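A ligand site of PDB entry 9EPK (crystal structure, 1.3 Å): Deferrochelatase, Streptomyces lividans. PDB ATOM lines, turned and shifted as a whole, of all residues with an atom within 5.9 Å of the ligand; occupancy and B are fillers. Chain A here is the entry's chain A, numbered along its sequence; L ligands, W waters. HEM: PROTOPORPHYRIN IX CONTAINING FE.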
ATOM      1  N   ASN A 186      16.569  16.360   1.614  1.00  0.00           N
ATOM      2  CA  ASN A 186      15.261  16.932   1.908  1.00  0.00           C
ATOM      3  C   ASN A 186      15.136  18.291   1.205  1.00  0.00           C
ATOM      4  O   ASN A 186      16.075  18.735   0.545  1.00  0.00           O
ATOM      5  CB  ASN A 186      15.009  16.989   3.419  1.00  0.00           C
ATOM      6  CG  ASN A 186      16.049  17.819   4.129  1.00  0.00           C
ATOM      7  OD1 ASN A 186      16.453  18.890   3.668  1.00  0.00           O
ATOM      8  ND2 ASN A 186      16.543  17.323   5.258  1.00  0.00           N
ATOM      9  N   LEU A 188      15.113  21.217   2.379  1.00  0.00           N
ATOM     10  CA  LEU A 188      16.027  22.236   2.871  1.00  0.00           C
ATOM     11  C   LEU A 188      17.385  22.133   2.191  1.00  0.00           C
ATOM     12  O   LEU A 188      18.267  22.949   2.429  1.00  0.00           O
ATOM     13  CB  LEU A 188      16.161  22.174   4.371  1.00  0.00           C
ATOM     14  CG  LEU A 188      14.875  22.338   5.141  1.00  0.00           C
ATOM     15  CD1 LEU A 188      15.177  22.421   6.635  1.00  0.00           C
ATOM     16  CD2 LEU A 188      14.078  23.552   4.702  1.00  0.00           C
ATOM     17  N   PHE A 190      19.636  19.537   2.483  1.00  0.00           N
ATOM     18  CA  PHE A 190      20.636  18.755   3.210  1.00  0.00           C
ATOM     19  C   PHE A 190      20.330  17.293   3.026  1.00  0.00           C
ATOM     20  O   PHE A 190      19.193  16.863   2.981  1.00  0.00           O
ATOM     21  CB  PHE A 190      20.544  19.097   4.694  1.00  0.00           C
ATOM     22  CG  PHE A 190      21.288  20.351   5.049  1.00  0.00           C
ATOM     23  CD1 PHE A 190      20.788  21.617   4.782  1.00  0.00           C
ATOM     24  CD2 PHE A 190      22.545  20.287   5.639  1.00  0.00           C
ATOM     25  CE1 PHE A 190      21.512  22.741   5.090  1.00  0.00           C
ATOM     26  CE2 PHE A 190      23.259  21.432   5.948  1.00  0.00           C
ATOM     27  CZ  PHE A 190      22.758  22.639   5.669  1.00  0.00           C
ATOM     28  N   LYS A 191      21.410  16.507   2.983  1.00  0.00           N
ATOM     29  CA  LYS A 191      21.332  15.059   3.034  1.00  0.00           C
ATOM     30  C   LYS A 191      20.637  14.650   4.323  1.00  0.00           C
ATOM     31  O   LYS A 191      20.933  15.218   5.387  1.00  0.00           O
ATOM     32  CB  LYS A 191      22.723  14.412   3.016  1.00  0.00           C
ATOM     33  CG  LYS A 191      23.455  14.631   1.719  1.00  0.00           C
ATOM     34  CD  LYS A 191      24.863  14.012   1.802  1.00  0.00           C
ATOM     35  CE  LYS A 191      25.604  14.132   0.505  1.00  0.00           C
ATOM     36  NZ  LYS A 191      26.990  13.644   0.632  1.00  0.00           N
ATOM     37  N   ASP A 192      19.759  13.680   4.256  1.00  0.00           N
ATOM     38  CA  ASP A 192      18.930  13.263   5.376  1.00  0.00           C
ATOM     39  C   ASP A 192      18.921  11.742   5.327  1.00  0.00           C
ATOM     40  O   ASP A 192      18.369  11.154   4.415  1.00  0.00           O
ATOM     41  CB  ASP A 192      17.534  13.874   5.266  1.00  0.00           C
ATOM     42  CG  ASP A 192      16.735  13.965   6.532  1.00  0.00           C
ATOM     43  OD1 ASP A 192      17.043  13.338   7.537  1.00  0.00           O
ATOM     44  OD2 ASP A 192      15.816  14.803   6.510  1.00  0.00           O
ATOM     45  N   GLY A 193      19.537  11.131   6.348  1.00  0.00           N
ATOM     46  CA  GLY A 193      19.604   9.681   6.464  1.00  0.00           C
ATOM     47  C   GLY A 193      21.008   9.147   6.680  1.00  0.00           C
ATOM     48  O   GLY A 193      21.140   7.934   6.779  1.00  0.00           O
ATOM     49  N   THR A 194      22.030   9.984   6.790  1.00  0.00           N
ATOM     50  CA  THR A 194      23.387   9.491   6.921  1.00  0.00           C
ATOM     51  C   THR A 194      23.522   8.550   8.110  1.00  0.00           C
ATOM     52  O   THR A 194      24.057   7.448   7.971  1.00  0.00           O
ATOM     53  CB  THR A 194      24.320  10.685   7.058  1.00  0.00           C
ATOM     54  OG1 THR A 194      24.142  11.511   5.921  1.00  0.00           O
ATOM     55  CG2 THR A 194      25.774  10.259   7.220  1.00  0.00           C
ATOM     56  N   ARG A 195      23.133   8.993   9.306  1.00  0.00           N
ATOM     57  CA  ARG A 195      23.285   8.191  10.507  1.00  0.00           C
ATOM     58  C   ARG A 195      21.945   7.660  10.939  1.00  0.00           C
ATOM     59  O   ARG A 195      21.275   8.229  11.789  1.00  0.00           O
ATOM     60  CB  ARG A 195      23.972   8.984  11.612  1.00  0.00           C
ATOM     61  CG  ARG A 195      25.503   8.971  11.495  1.00  0.00           C
ATOM     62  CD  ARG A 195      26.233   9.777  12.531  1.00  0.00           C
ATOM     63  NE  ARG A 195      25.691   9.559  13.859  1.00  0.00           N
ATOM     64  CZ  ARG A 195      25.738   8.446  14.547  1.00  0.00           C
ATOM     65  NH1 ARG A 195      24.890   8.298  15.517  1.00  0.00           N
ATOM     66  NH2 ARG A 195      26.602   7.486  14.233  1.00  0.00           N
ATOM     67  N   ASN A 196      21.527   6.585  10.270  1.00  0.00           N
ATOM     68  CA  ASN A 196      20.287   5.897  10.512  1.00  0.00           C
ATOM     69  C   ASN A 196      20.623   4.505  11.027  1.00  0.00           C
ATOM     70  O   ASN A 196      21.546   4.347  11.853  1.00  0.00           O
ATOM     71  CB  ASN A 196      19.401   6.048   9.286  1.00  0.00           C
ATOM     72  CG  ASN A 196      17.974   5.749   9.585  1.00  0.00           C
ATOM     73  OD1 ASN A 196      17.445   6.086  10.642  1.00  0.00           O
ATOM     74  ND2 ASN A 196      17.278   5.140   8.668  1.00  0.00           N
ATOM     75  N   ARG A 229       4.849  12.058  11.834  1.00  0.00           N
ATOM     76  CA  ARG A 229       4.662  13.485  12.074  1.00  0.00           C
ATOM     77  C   ARG A 229       4.677  14.196  10.749  1.00  0.00           C
ATOM     78  O   ARG A 229       5.626  14.090   9.966  1.00  0.00           O
ATOM     79  CB  ARG A 229       5.752  14.082  12.970  1.00  0.00           C
ATOM     80  CG  ARG A 229       5.864  13.422  14.336  1.00  0.00           C
ATOM     81  CD  ARG A 229       4.761  13.704  15.300  1.00  0.00           C
ATOM     82  NE  ARG A 229       4.989  15.072  15.786  1.00  0.00           N
ATOM     83  CZ  ARG A 229       4.445  15.576  16.889  1.00  0.00           C
ATOM     84  NH1 ARG A 229       3.530  14.942  17.548  1.00  0.00           N
ATOM     85  NH2 ARG A 229       4.824  16.770  17.298  1.00  0.00           N
ATOM     86  N   ILE A 231       5.276  17.529   8.991  1.00  0.00           N
ATOM     87  CA  ILE A 231       6.045  18.704   9.381  1.00  0.00           C
ATOM     88  C   ILE A 231       6.070  19.663   8.212  1.00  0.00           C
ATOM     89  O   ILE A 231       6.605  19.368   7.144  1.00  0.00           O
ATOM     90  CB  ILE A 231       7.449  18.307   9.810  1.00  0.00           C
ATOM     91  CG1 ILE A 231       7.420  17.267  10.894  1.00  0.00           C
ATOM     92  CG2 ILE A 231       8.216  19.552  10.256  1.00  0.00           C
ATOM     93  CD1 ILE A 231       8.773  16.730  11.293  1.00  0.00           C
ATOM     94  N   MET A 233       7.486  22.964   6.431  1.00  0.00           N
ATOM     95  CA  MET A 233       8.739  23.711   6.398  1.00  0.00           C
ATOM     96  C   MET A 233       8.458  25.134   5.964  1.00  0.00           C
ATOM     97  O   MET A 233       7.760  25.381   5.001  1.00  0.00           O
ATOM     98  CB  MET A 233       9.693  23.078   5.376  1.00  0.00           C
ATOM     99  CG  MET A 233      10.234  21.734   5.805  1.00  0.00           C
ATOM    100  SD  MET A 233      11.082  20.945   4.388  1.00  0.00           S
ATOM    101  CE  MET A 233      12.119  19.715   5.174  1.00  0.00           C
ATOM    102  N   PHE A 250      22.205  22.667  11.456  1.00  0.00           N
ATOM    103  CA  PHE A 250      22.330  21.220  11.453  1.00  0.00           C
ATOM    104  C   PHE A 250      23.578  20.699  12.149  1.00  0.00           C
ATOM    105  O   PHE A 250      23.523  19.645  12.786  1.00  0.00           O
ATOM    106  CB  PHE A 250      22.265  20.696  10.021  1.00  0.00           C
ATOM    107  CG  PHE A 250      20.833  20.695   9.528  1.00  0.00           C
ATOM    108  CD1 PHE A 250      19.895  19.886  10.126  1.00  0.00           C
ATOM    109  CD2 PHE A 250      20.442  21.537   8.492  1.00  0.00           C
ATOM    110  CE1 PHE A 250      18.563  19.945   9.732  1.00  0.00           C
ATOM    111  CE2 PHE A 250      19.104  21.559   8.095  1.00  0.00           C
ATOM    112  CZ  PHE A 250      18.186  20.772   8.737  1.00  0.00           C
ATOM    113  N   ARG A 252      26.244  20.087  10.116  1.00  0.00           N
ATOM    114  CA  ARG A 252      26.867  19.453   8.974  1.00  0.00           C
ATOM    115  C   ARG A 252      26.941  20.490   7.868  1.00  0.00           C
ATOM    116  O   ARG A 252      26.119  21.391   7.845  1.00  0.00           O
ATOM    117  CB  ARG A 252      26.110  18.219   8.487  1.00  0.00           C
ATOM    118  CG  ARG A 252      26.214  17.072   9.468  1.00  0.00           C
ATOM    119  CD  ARG A 252      25.379  15.866   9.003  1.00  0.00           C
ATOM    120  NE  ARG A 252      25.525  14.673   9.825  1.00  0.00           N
ATOM    121  CZ  ARG A 252      26.404  13.711   9.605  1.00  0.00           C
ATOM    122  NH1 ARG A 252      27.336  13.787   8.663  1.00  0.00           N
ATOM    123  NH2 ARG A 252      26.358  12.658  10.384  1.00  0.00           N
ATOM    124  N   PRO A 269      30.426  12.339  13.698  1.00  0.00           N
ATOM    125  CA  PRO A 269      30.341  13.658  14.279  1.00  0.00           C
ATOM    126  C   PRO A 269      31.188  13.813  15.527  1.00  0.00           C
ATOM    127  O   PRO A 269      31.248  12.915  16.340  1.00  0.00           O
ATOM    128  CB  PRO A 269      28.845  13.848  14.606  1.00  0.00           C
ATOM    129  CG  PRO A 269      28.166  12.636  14.089  1.00  0.00           C
ATOM    130  CD  PRO A 269      29.158  11.601  13.624  1.00  0.00           C
ATOM    131  N   HIS A 279      20.792  20.704  15.337  1.00  0.00           N
ATOM    132  CA  HIS A 279      19.900  19.562  15.227  1.00  0.00           C
ATOM    133  C   HIS A 279      20.613  18.228  15.447  1.00  0.00           C
ATOM    134  O   HIS A 279      20.144  17.407  16.201  1.00  0.00           O
ATOM    135  CB  HIS A 279      19.204  19.603  13.871  1.00  0.00           C
ATOM    136  CG  HIS A 279      18.259  18.493  13.646  1.00  0.00           C
ATOM    137  ND1 HIS A 279      17.044  18.448  14.238  1.00  0.00           N
ATOM    138  CD2 HIS A 279      18.343  17.375  12.863  1.00  0.00           C
ATOM    139  CE1 HIS A 279      16.406  17.345  13.805  1.00  0.00           C
ATOM    140  NE2 HIS A 279      17.159  16.675  12.977  1.00  0.00           N
ATOM    141  N   VAL A 280      21.767  18.012  14.784  1.00  0.00           N
ATOM    142  CA  VAL A 280      22.466  16.745  14.908  1.00  0.00           C
ATOM    143  C   VAL A 280      22.940  16.530  16.346  1.00  0.00           C
ATOM    144  O   VAL A 280      22.845  15.423  16.877  1.00  0.00           O
ATOM    145  CB  VAL A 280      23.605  16.614  13.900  1.00  0.00           C
ATOM    146  CG1 VAL A 280      24.467  15.420  14.236  1.00  0.00           C
ATOM    147  CG2 VAL A 280      23.015  16.514  12.493  1.00  0.00           C
ATOM    148  N   ALA A 283      19.919  15.580  18.474  1.00  0.00           N
ATOM    149  CA  ALA A 283      19.205  14.366  18.109  1.00  0.00           C
ATOM    150  C   ALA A 283      20.075  13.137  18.233  1.00  0.00           C
ATOM    151  O   ALA A 283      19.575  12.019  18.164  1.00  0.00           O
ATOM    152  CB  ALA A 283      18.765  14.484  16.659  1.00  0.00           C
ATOM    153  N   HIS A 284      21.402  13.300  18.355  1.00  0.00           N
ATOM    154  CA  HIS A 284      22.336  12.186  18.327  1.00  0.00           C
ATOM    155  C   HIS A 284      22.076  11.259  19.493  1.00  0.00           C
ATOM    156  O   HIS A 284      21.766  11.752  20.585  1.00  0.00           O
ATOM    157  CB  HIS A 284      23.768  12.707  18.438  1.00  0.00           C
ATOM    158  CG  HIS A 284      24.835  11.753  18.103  1.00  0.00           C
ATOM    159  ND1 HIS A 284      25.272  10.810  19.009  1.00  0.00           N
ATOM    160  CD2 HIS A 284      25.589  11.618  17.024  1.00  0.00           C
ATOM    161  CE1 HIS A 284      26.257  10.124  18.465  1.00  0.00           C
ATOM    162  NE2 HIS A 284      26.502  10.585  17.251  1.00  0.00           N
ATOM    163  N   PRO A 285      22.208   9.925  19.332  1.00  0.00           N
ATOM    164  CA  PRO A 285      22.021   8.989  20.452  1.00  0.00           C
ATOM    165  C   PRO A 285      22.838   9.347  21.692  1.00  0.00           C
ATOM    166  O   PRO A 285      22.297   9.215  22.802  1.00  0.00           O
ATOM    167  CB  PRO A 285      22.489   7.658  19.856  1.00  0.00           C
ATOM    168  CG  PRO A 285      22.155   7.770  18.412  1.00  0.00           C
ATOM    169  CD  PRO A 285      22.470   9.202  18.089  1.00  0.00           C
ATOM    170  N   LEU A 293      16.767   5.742  16.543  1.00  0.00           N
ATOM    171  CA  LEU A 293      15.536   5.547  15.771  1.00  0.00           C
ATOM    172  C   LEU A 293      15.839   5.050  14.379  1.00  0.00           C
ATOM    173  O   LEU A 293      16.930   5.254  13.900  1.00  0.00           O
ATOM    174  CB  LEU A 293      14.923   6.933  15.505  1.00  0.00           C
ATOM    175  CG  LEU A 293      14.641   7.828  16.694  1.00  0.00           C
ATOM    176  CD1 LEU A 293      14.104   9.197  16.293  1.00  0.00           C
ATOM    177  CD2 LEU A 293      13.606   7.140  17.545  1.00  0.00           C
ATOM    178  N   ARG A 295      14.628   6.099  10.982  1.00  0.00           N
ATOM    179  CA  ARG A 295      13.905   7.144  10.266  1.00  0.00           C
ATOM    180  C   ARG A 295      13.624   6.699   8.847  1.00  0.00           C
ATOM    181  O   ARG A 295      14.514   6.166   8.187  1.00  0.00           O
ATOM    182  CB  ARG A 295      14.741   8.429  10.243  1.00  0.00           C
ATOM    183  CG  ARG A 295      14.892   9.079  11.601  1.00  0.00           C
ATOM    184  CD  ARG A 295      15.793  10.245  11.589  1.00  0.00           C
ATOM    185  NE  ARG A 295      17.165   9.815  11.398  1.00  0.00           N
ATOM    186  CZ  ARG A 295      18.068  10.404  10.663  1.00  0.00           C
ATOM    187  NH1 ARG A 295      17.801  11.430   9.918  1.00  0.00           N
ATOM    188  NH2 ARG A 295      19.285   9.887  10.607  1.00  0.00           N
ATOM    189  N   LEU A 314       7.856  17.736   5.214  1.00  0.00           N
ATOM    190  CA  LEU A 314       8.458  16.432   5.392  1.00  0.00           C
ATOM    191  C   LEU A 314       7.495  15.620   6.206  1.00  0.00           C
ATOM    192  O   LEU A 314       7.030  16.051   7.250  1.00  0.00           O
ATOM    193  CB  LEU A 314       9.828  16.642   6.048  1.00  0.00           C
ATOM    194  CG  LEU A 314      10.796  15.457   5.982  1.00  0.00           C
ATOM    195  CD1 LEU A 314      12.239  15.859   6.029  1.00  0.00           C
ATOM    196  CD2 LEU A 314      10.537  14.503   7.096  1.00  0.00           C
ATOM    197  N   PHE A 316       7.556  12.794   8.354  1.00  0.00           N
ATOM    198  CA  PHE A 316       8.538  12.113   9.174  1.00  0.00           C
ATOM    199  C   PHE A 316       7.947  10.821   9.698  1.00  0.00           C
ATOM    200  O   PHE A 316       6.885  10.802  10.266  1.00  0.00           O
ATOM    201  CB  PHE A 316       8.893  13.057  10.325  1.00  0.00           C
ATOM    202  CG  PHE A 316       9.955  12.490  11.243  1.00  0.00           C
ATOM    203  CD1 PHE A 316      11.294  12.676  10.939  1.00  0.00           C
ATOM    204  CD2 PHE A 316       9.613  11.775  12.346  1.00  0.00           C
ATOM    205  CE1 PHE A 316      12.270  12.138  11.771  1.00  0.00           C
ATOM    206  CE2 PHE A 316      10.605  11.289  13.172  1.00  0.00           C
ATOM    207  CZ  PHE A 316      11.910  11.439  12.856  1.00  0.00           C
ATOM    208  N   PHE A 327      11.247   7.875  20.004  1.00  0.00           N
ATOM    209  CA  PHE A 327      10.877   9.204  19.550  1.00  0.00           C
ATOM    210  C   PHE A 327      10.716  10.185  20.710  1.00  0.00           C
ATOM    211  O   PHE A 327      11.107  11.338  20.567  1.00  0.00           O
ATOM    212  CB  PHE A 327       9.571   9.083  18.768  1.00  0.00           C
ATOM    213  CG  PHE A 327       9.027  10.405  18.266  1.00  0.00           C
ATOM    214  CD1 PHE A 327       9.568  10.996  17.144  1.00  0.00           C
ATOM    215  CD2 PHE A 327       8.079  11.149  18.973  1.00  0.00           C
ATOM    216  CE1 PHE A 327       9.132  12.216  16.696  1.00  0.00           C
ATOM    217  CE2 PHE A 327       7.632  12.357  18.487  1.00  0.00           C
ATOM    218  CZ  PHE A 327       8.193  12.911  17.396  1.00  0.00           C
ATOM    219  N   VAL A 330      13.931  11.804  22.135  1.00  0.00           N
ATOM    220  CA  VAL A 330      14.666  12.574  21.159  1.00  0.00           C
ATOM    221  C   VAL A 330      13.877  13.844  20.841  1.00  0.00           C
ATOM    222  O   VAL A 330      14.439  14.929  20.852  1.00  0.00           O
ATOM    223  CB  VAL A 330      14.944  11.715  19.908  1.00  0.00           C
ATOM    224  CG1 VAL A 330      15.571  12.559  18.825  1.00  0.00           C
ATOM    225  CG2 VAL A 330      15.845  10.528  20.258  1.00  0.00           C
ATOM    226  N   GLN A 331      12.570  13.750  20.596  1.00  0.00           N
ATOM    227  CA  GLN A 331      11.774  14.945  20.329  1.00  0.00           C
ATOM    228  C   GLN A 331      11.772  15.914  21.503  1.00  0.00           C
ATOM    229  O   GLN A 331      11.782  17.137  21.310  1.00  0.00           O
ATOM    230  CB  GLN A 331      10.351  14.561  19.931  1.00  0.00           C
ATOM    231  CG  GLN A 331       9.440  15.733  19.589  1.00  0.00           C
ATOM    232  CD  GLN A 331       9.895  16.590  18.452  1.00  0.00           C
ATOM    233  OE1 GLN A 331      10.521  16.134  17.503  1.00  0.00           O
ATOM    234  NE2 GLN A 331       9.598  17.868  18.512  1.00  0.00           N
ATOM    235  N   LEU A 334      14.654  18.040  21.348  1.00  0.00           N
ATOM    236  CA  LEU A 334      14.639  19.010  20.275  1.00  0.00           C
ATOM    237  C   LEU A 334      13.867  20.269  20.650  1.00  0.00           C
ATOM    238  O   LEU A 334      13.664  21.152  19.819  1.00  0.00           O
ATOM    239  CB  LEU A 334      14.100  18.392  18.990  1.00  0.00           C
ATOM    240  CG  LEU A 334      14.868  17.189  18.460  1.00  0.00           C
ATOM    241  CD1 LEU A 334      14.281  16.708  17.118  1.00  0.00           C
ATOM    242  CD2 LEU A 334      16.307  17.483  18.246  1.00  0.00           C
ATOM    243  N   LEU A 339      16.537  24.211  14.427  1.00  0.00           N
ATOM    244  CA  LEU A 339      15.645  23.906  13.316  1.00  0.00           C
ATOM    245  C   LEU A 339      14.203  24.334  13.587  1.00  0.00           C
ATOM    246  O   LEU A 339      13.471  24.580  12.652  1.00  0.00           O
ATOM    247  CB  LEU A 339      15.725  22.396  13.053  1.00  0.00           C
ATOM    248  CG  LEU A 339      14.926  21.887  11.853  1.00  0.00           C
ATOM    249  CD1 LEU A 339      15.350  22.493  10.549  1.00  0.00           C
ATOM    250  CD2 LEU A 339      14.980  20.381  11.793  1.00  0.00           C
ATOM    251  N   ILE A 343      10.337  25.091  11.034  1.00  0.00           N
ATOM    252  CA  ILE A 343       9.421  23.956  10.878  1.00  0.00           C
ATOM    253  C   ILE A 343       8.243  24.103  11.812  1.00  0.00           C
ATOM    254  O   ILE A 343       8.296  24.856  12.772  1.00  0.00           O
ATOM    255  CB  ILE A 343      10.088  22.592  11.080  1.00  0.00           C
ATOM    256  CG1 ILE A 343      10.589  22.415  12.499  1.00  0.00           C
ATOM    257  CG2 ILE A 343      11.191  22.361  10.061  1.00  0.00           C
ATOM    258  CD1 ILE A 343      10.968  20.982  12.842  1.00  0.00           C
ATOM    259  N   HIS A 345       5.269  21.172  13.391  1.00  0.00           N
ATOM    260  CA  HIS A 345       4.559  19.900  13.304  1.00  0.00           C
ATOM    261  C   HIS A 345       3.077  20.175  13.250  1.00  0.00           C
ATOM    262  O   HIS A 345       2.533  20.831  14.158  1.00  0.00           O
ATOM    263  CB  HIS A 345       4.887  19.060  14.517  1.00  0.00           C
ATOM    264  CG  HIS A 345       6.302  18.592  14.593  1.00  0.00           C
ATOM    265  ND1 HIS A 345       6.634  17.282  14.802  1.00  0.00           N
ATOM    266  CD2 HIS A 345       7.480  19.289  14.594  1.00  0.00           C
ATOM    267  CE1 HIS A 345       7.948  17.181  14.886  1.00  0.00           C
ATOM    268  NE2 HIS A 345       8.489  18.395  14.784  1.00  0.00           N
HETATM  269  CHA HEM L   1      19.694  13.851  11.525  1.00  0.00           C
HETATM  270  CHB HEM L   1      17.057  17.008   8.992  1.00  0.00           C
HETATM  271  CHC HEM L   1      13.296  16.177  11.879  1.00  0.00           C
HETATM  272  CHD HEM L   1      15.922  12.951  14.316  1.00  0.00           C
HETATM  273  C1A HEM L   1      19.349  14.803  10.583  1.00  0.00           C
HETATM  274  C2A HEM L   1      20.206  15.320   9.568  1.00  0.00           C
HETATM  275  C3A HEM L   1      19.489  16.224   8.872  1.00  0.00           C
HETATM  276  C4A HEM L   1      18.160  16.242   9.453  1.00  0.00           C
HETATM  277  CMA HEM L   1      19.882  17.079   7.722  1.00  0.00           C
HETATM  278  CAA HEM L   1      21.663  14.968   9.388  1.00  0.00           C
HETATM  279  CBA HEM L   1      21.907  13.732   8.491  1.00  0.00           C
HETATM  280  CGA HEM L   1      21.470  12.477   9.090  1.00  0.00           C
HETATM  281  O1A HEM L   1      20.341  12.014   8.788  1.00  0.00           O
HETATM  282  O2A HEM L   1      22.240  11.863   9.879  1.00  0.00           O
HETATM  283  C1B HEM L   1      15.787  17.033   9.565  1.00  0.00           C
HETATM  284  C2B HEM L   1      14.704  17.840   9.055  1.00  0.00           C
HETATM  285  C3B HEM L   1      13.646  17.616   9.848  1.00  0.00           C
HETATM  286  C4B HEM L   1      14.080  16.656  10.871  1.00  0.00           C
HETATM  287  CMB HEM L   1      14.749  18.744   7.885  1.00  0.00           C
HETATM  288  CAB HEM L   1      12.260  18.135   9.806  1.00  0.00           C
HETATM  289  CBB HEM L   1      11.722  18.716   8.808  1.00  0.00           C
HETATM  290  C1C HEM L   1      13.658  15.257  12.829  1.00  0.00           C
HETATM  291  C2C HEM L   1      12.867  14.738  13.880  1.00  0.00           C
HETATM  292  C3C HEM L   1      13.602  13.817  14.592  1.00  0.00           C
HETATM  293  C4C HEM L   1      14.872  13.791  13.941  1.00  0.00           C
HETATM  294  CMC HEM L   1      11.444  15.129  14.104  1.00  0.00           C
HETATM  295  CAC HEM L   1      13.283  13.013  15.788  1.00  0.00           C
HETATM  296  CBC HEM L   1      12.410  13.367  16.639  1.00  0.00           C
HETATM  297  C1D HEM L   1      17.176  12.897  13.689  1.00  0.00           C
HETATM  298  C2D HEM L   1      18.225  11.952  14.093  1.00  0.00           C
HETATM  299  C3D HEM L   1      19.283  12.229  13.325  1.00  0.00           C
HETATM  300  C4D HEM L   1      18.881  13.294  12.447  1.00  0.00           C
HETATM  301  CMD HEM L   1      18.055  10.907  15.179  1.00  0.00           C
HETATM  302  CAD HEM L   1      20.587  11.506  13.374  1.00  0.00           C
HETATM  303  CBD HEM L   1      21.565  12.124  14.411  1.00  0.00           C
HETATM  304  CGD HEM L   1      22.814  11.343  14.532  1.00  0.00           C
HETATM  305  O1D HEM L   1      23.845  11.792  14.006  1.00  0.00           O
HETATM  306  O2D HEM L   1      22.752  10.239  15.113  1.00  0.00           O
HETATM  307  NA  HEM L   1      18.079  15.373  10.464  1.00  0.00           N
HETATM  308  NB  HEM L   1      15.381  16.354  10.625  1.00  0.00           N
HETATM  309  NC  HEM L   1      14.889  14.647  12.895  1.00  0.00           N
HETATM  310  ND  HEM L   1      17.592  13.641  12.692  1.00  0.00           N
HETATM  311 FE   HEM L   1      16.556  15.091  11.743  1.00  0.00          FE
HETATM  312  O   HOH W   1      15.917  13.610  10.092  1.00  0.00           O
HETATM  313  O   HOH W   2      13.929  14.342   8.359  1.00  0.00           O
HETATM  314  O   HOH W   3      18.632   9.358  18.082  1.00  0.00           O
HETATM  315  O   HOH W   4      21.338   7.996  14.581  1.00  0.00           O
HETATM  316  O   HOH W   5      23.865  13.098  11.630  1.00  0.00           O
HETATM  317  O   HOH W   6      18.840   7.662  15.839  1.00  0.00           O
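FE of the ligand is bound by NE2 of His 279 (2.1 Å).
N of Gly 193 lies within hydrogen-bond range of O1A of the ligand (2.7 Å).
An oxygen (O1A) of the ligand lies within salt-bridge range of the guanidinium group of Arg 295 (2.8 Å).
O1A of the ligand is in hydrogen-bond range of N of Thr 194 (3.3 Å).
O2A of the ligand is in hydrogen-bond range of N of Arg 195, 3.1 Å away.
NE of Arg 195 is in salt-bridge range of O1D of the ligand, 2.9 Å away.
OD1 of Asn 186 is in hydrogen-bond range of N of Leu 188 (3.0 Å).
The side-chain carboxylate (OD2) of Asp 192 lies within hydrogen-bond range of the side-chain amide nitrogen (ND2) of Asn 186, at 2.9 Å.
N of Arg 295 is in hydrogen-bond range of OD1 of Asn 196, at 2.8 Å.
The guanidinium group of Arg 295 lies within salt-bridge range of the side-chain carboxylate of Asp 192.
The backbone carbonyl oxygen (O) of Arg 229 is in hydrogen-bond range of the backbone NH (N) of Phe 316, 2.8 Å away.
NH2 of Arg 295 lies within hydrogen-bond range of O of Arg 195 (2.8 Å).
NE2 of His 284 lies within hydrogen-bond range of NH1 of Arg 195 (3.3 Å).
The backbone NH (N) of Val 280 is in hydrogen-bond range of the backbone carbonyl oxygen (O) of Phe 250 (3.1 Å).
ND2 of Asn 186 touches CMB of the ligand, at 3.5 Å.
CD1 of Leu 188 touches CMB of the ligand, at 3.9 Å.
Phe 190 touches the ligand (CB to CMA, 3.7 Å).
Lys 191 touches the ligand (O to CMA, 3.2 Å).
Asp 192 touches the ligand (OD2 to CHB, 3.5 Å).
CG2 of Ile 231 touches CBB of the ligand (3.9 Å).
CE of Met 233 touches CBB of the ligand, at 3.8 Å.
Phe 250 touches the ligand.
Arg 252 touches the ligand (CD to CAA, 3.8 Å).
Val 280 touches the ligand (CG1 to O1D, 3.7 Å).
Ala 283 touches the ligand.
His 284 touches the ligand (CD2 to O1D, 3.5 Å).
Pro 285 touches the ligand.
CD1 of Leu 293 touches CAC of the ligand, 3.9 Å away.
CB of Leu 314 touches CBB of the ligand (3.9 Å).
Phe 316 touches the ligand (CZ to C3C, 3.4 Å).
Phe 327 touches the ligand.
Val 330 touches the ligand.
Gln 331 touches the ligand (OE1 to CBC, 3.5 Å).
Leu 334 touches the ligand.
CD2 of Leu 339 touches C3B of the ligand, at 3.6 Å.
Ile 343 touches the ligand.
Hydrophobic or aromatic side chains that line the ligand: Leu 188, Phe 190, Ile 231, Met 233, Phe 250, His 279, Val 280, Ala 283, His 284, Pro 285, Leu 293, Leu 314, Phe 316, Phe 327, Val 330, Leu 334, Leu 339 and Ile 343.
27 residues have an atom within 4 Å of the ligand: Asn 186, Leu 188, Phe 190, Lys 191, Asp 192, Gly 193, Thr 194, Arg 195, Ile 231, Met 233, Phe 250, Arg 252, His 279, Val 280, Ala 283, His 284, Pro 285, Leu 293, Arg 295, Leu 314, Phe 316, Phe 327, Val 330, Gln 331, Leu 334, Leu 339 and Ile 343.
Water W1 lies within hydrogen-bond range of the side-chain carboxylate (OD1) of Asp 192 (2.8 Å) and the guanidinium group (NH1) of Arg 295 (2.9 Å).
Water W5 lies within hydrogen-bond range of O2A of the ligand (2.7 Å) and NH2 of Arg 252 (2.8 Å).
Water W4 bridges O2D of the ligand (2.7 Å) and O of Arg 195 (2.8 Å).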
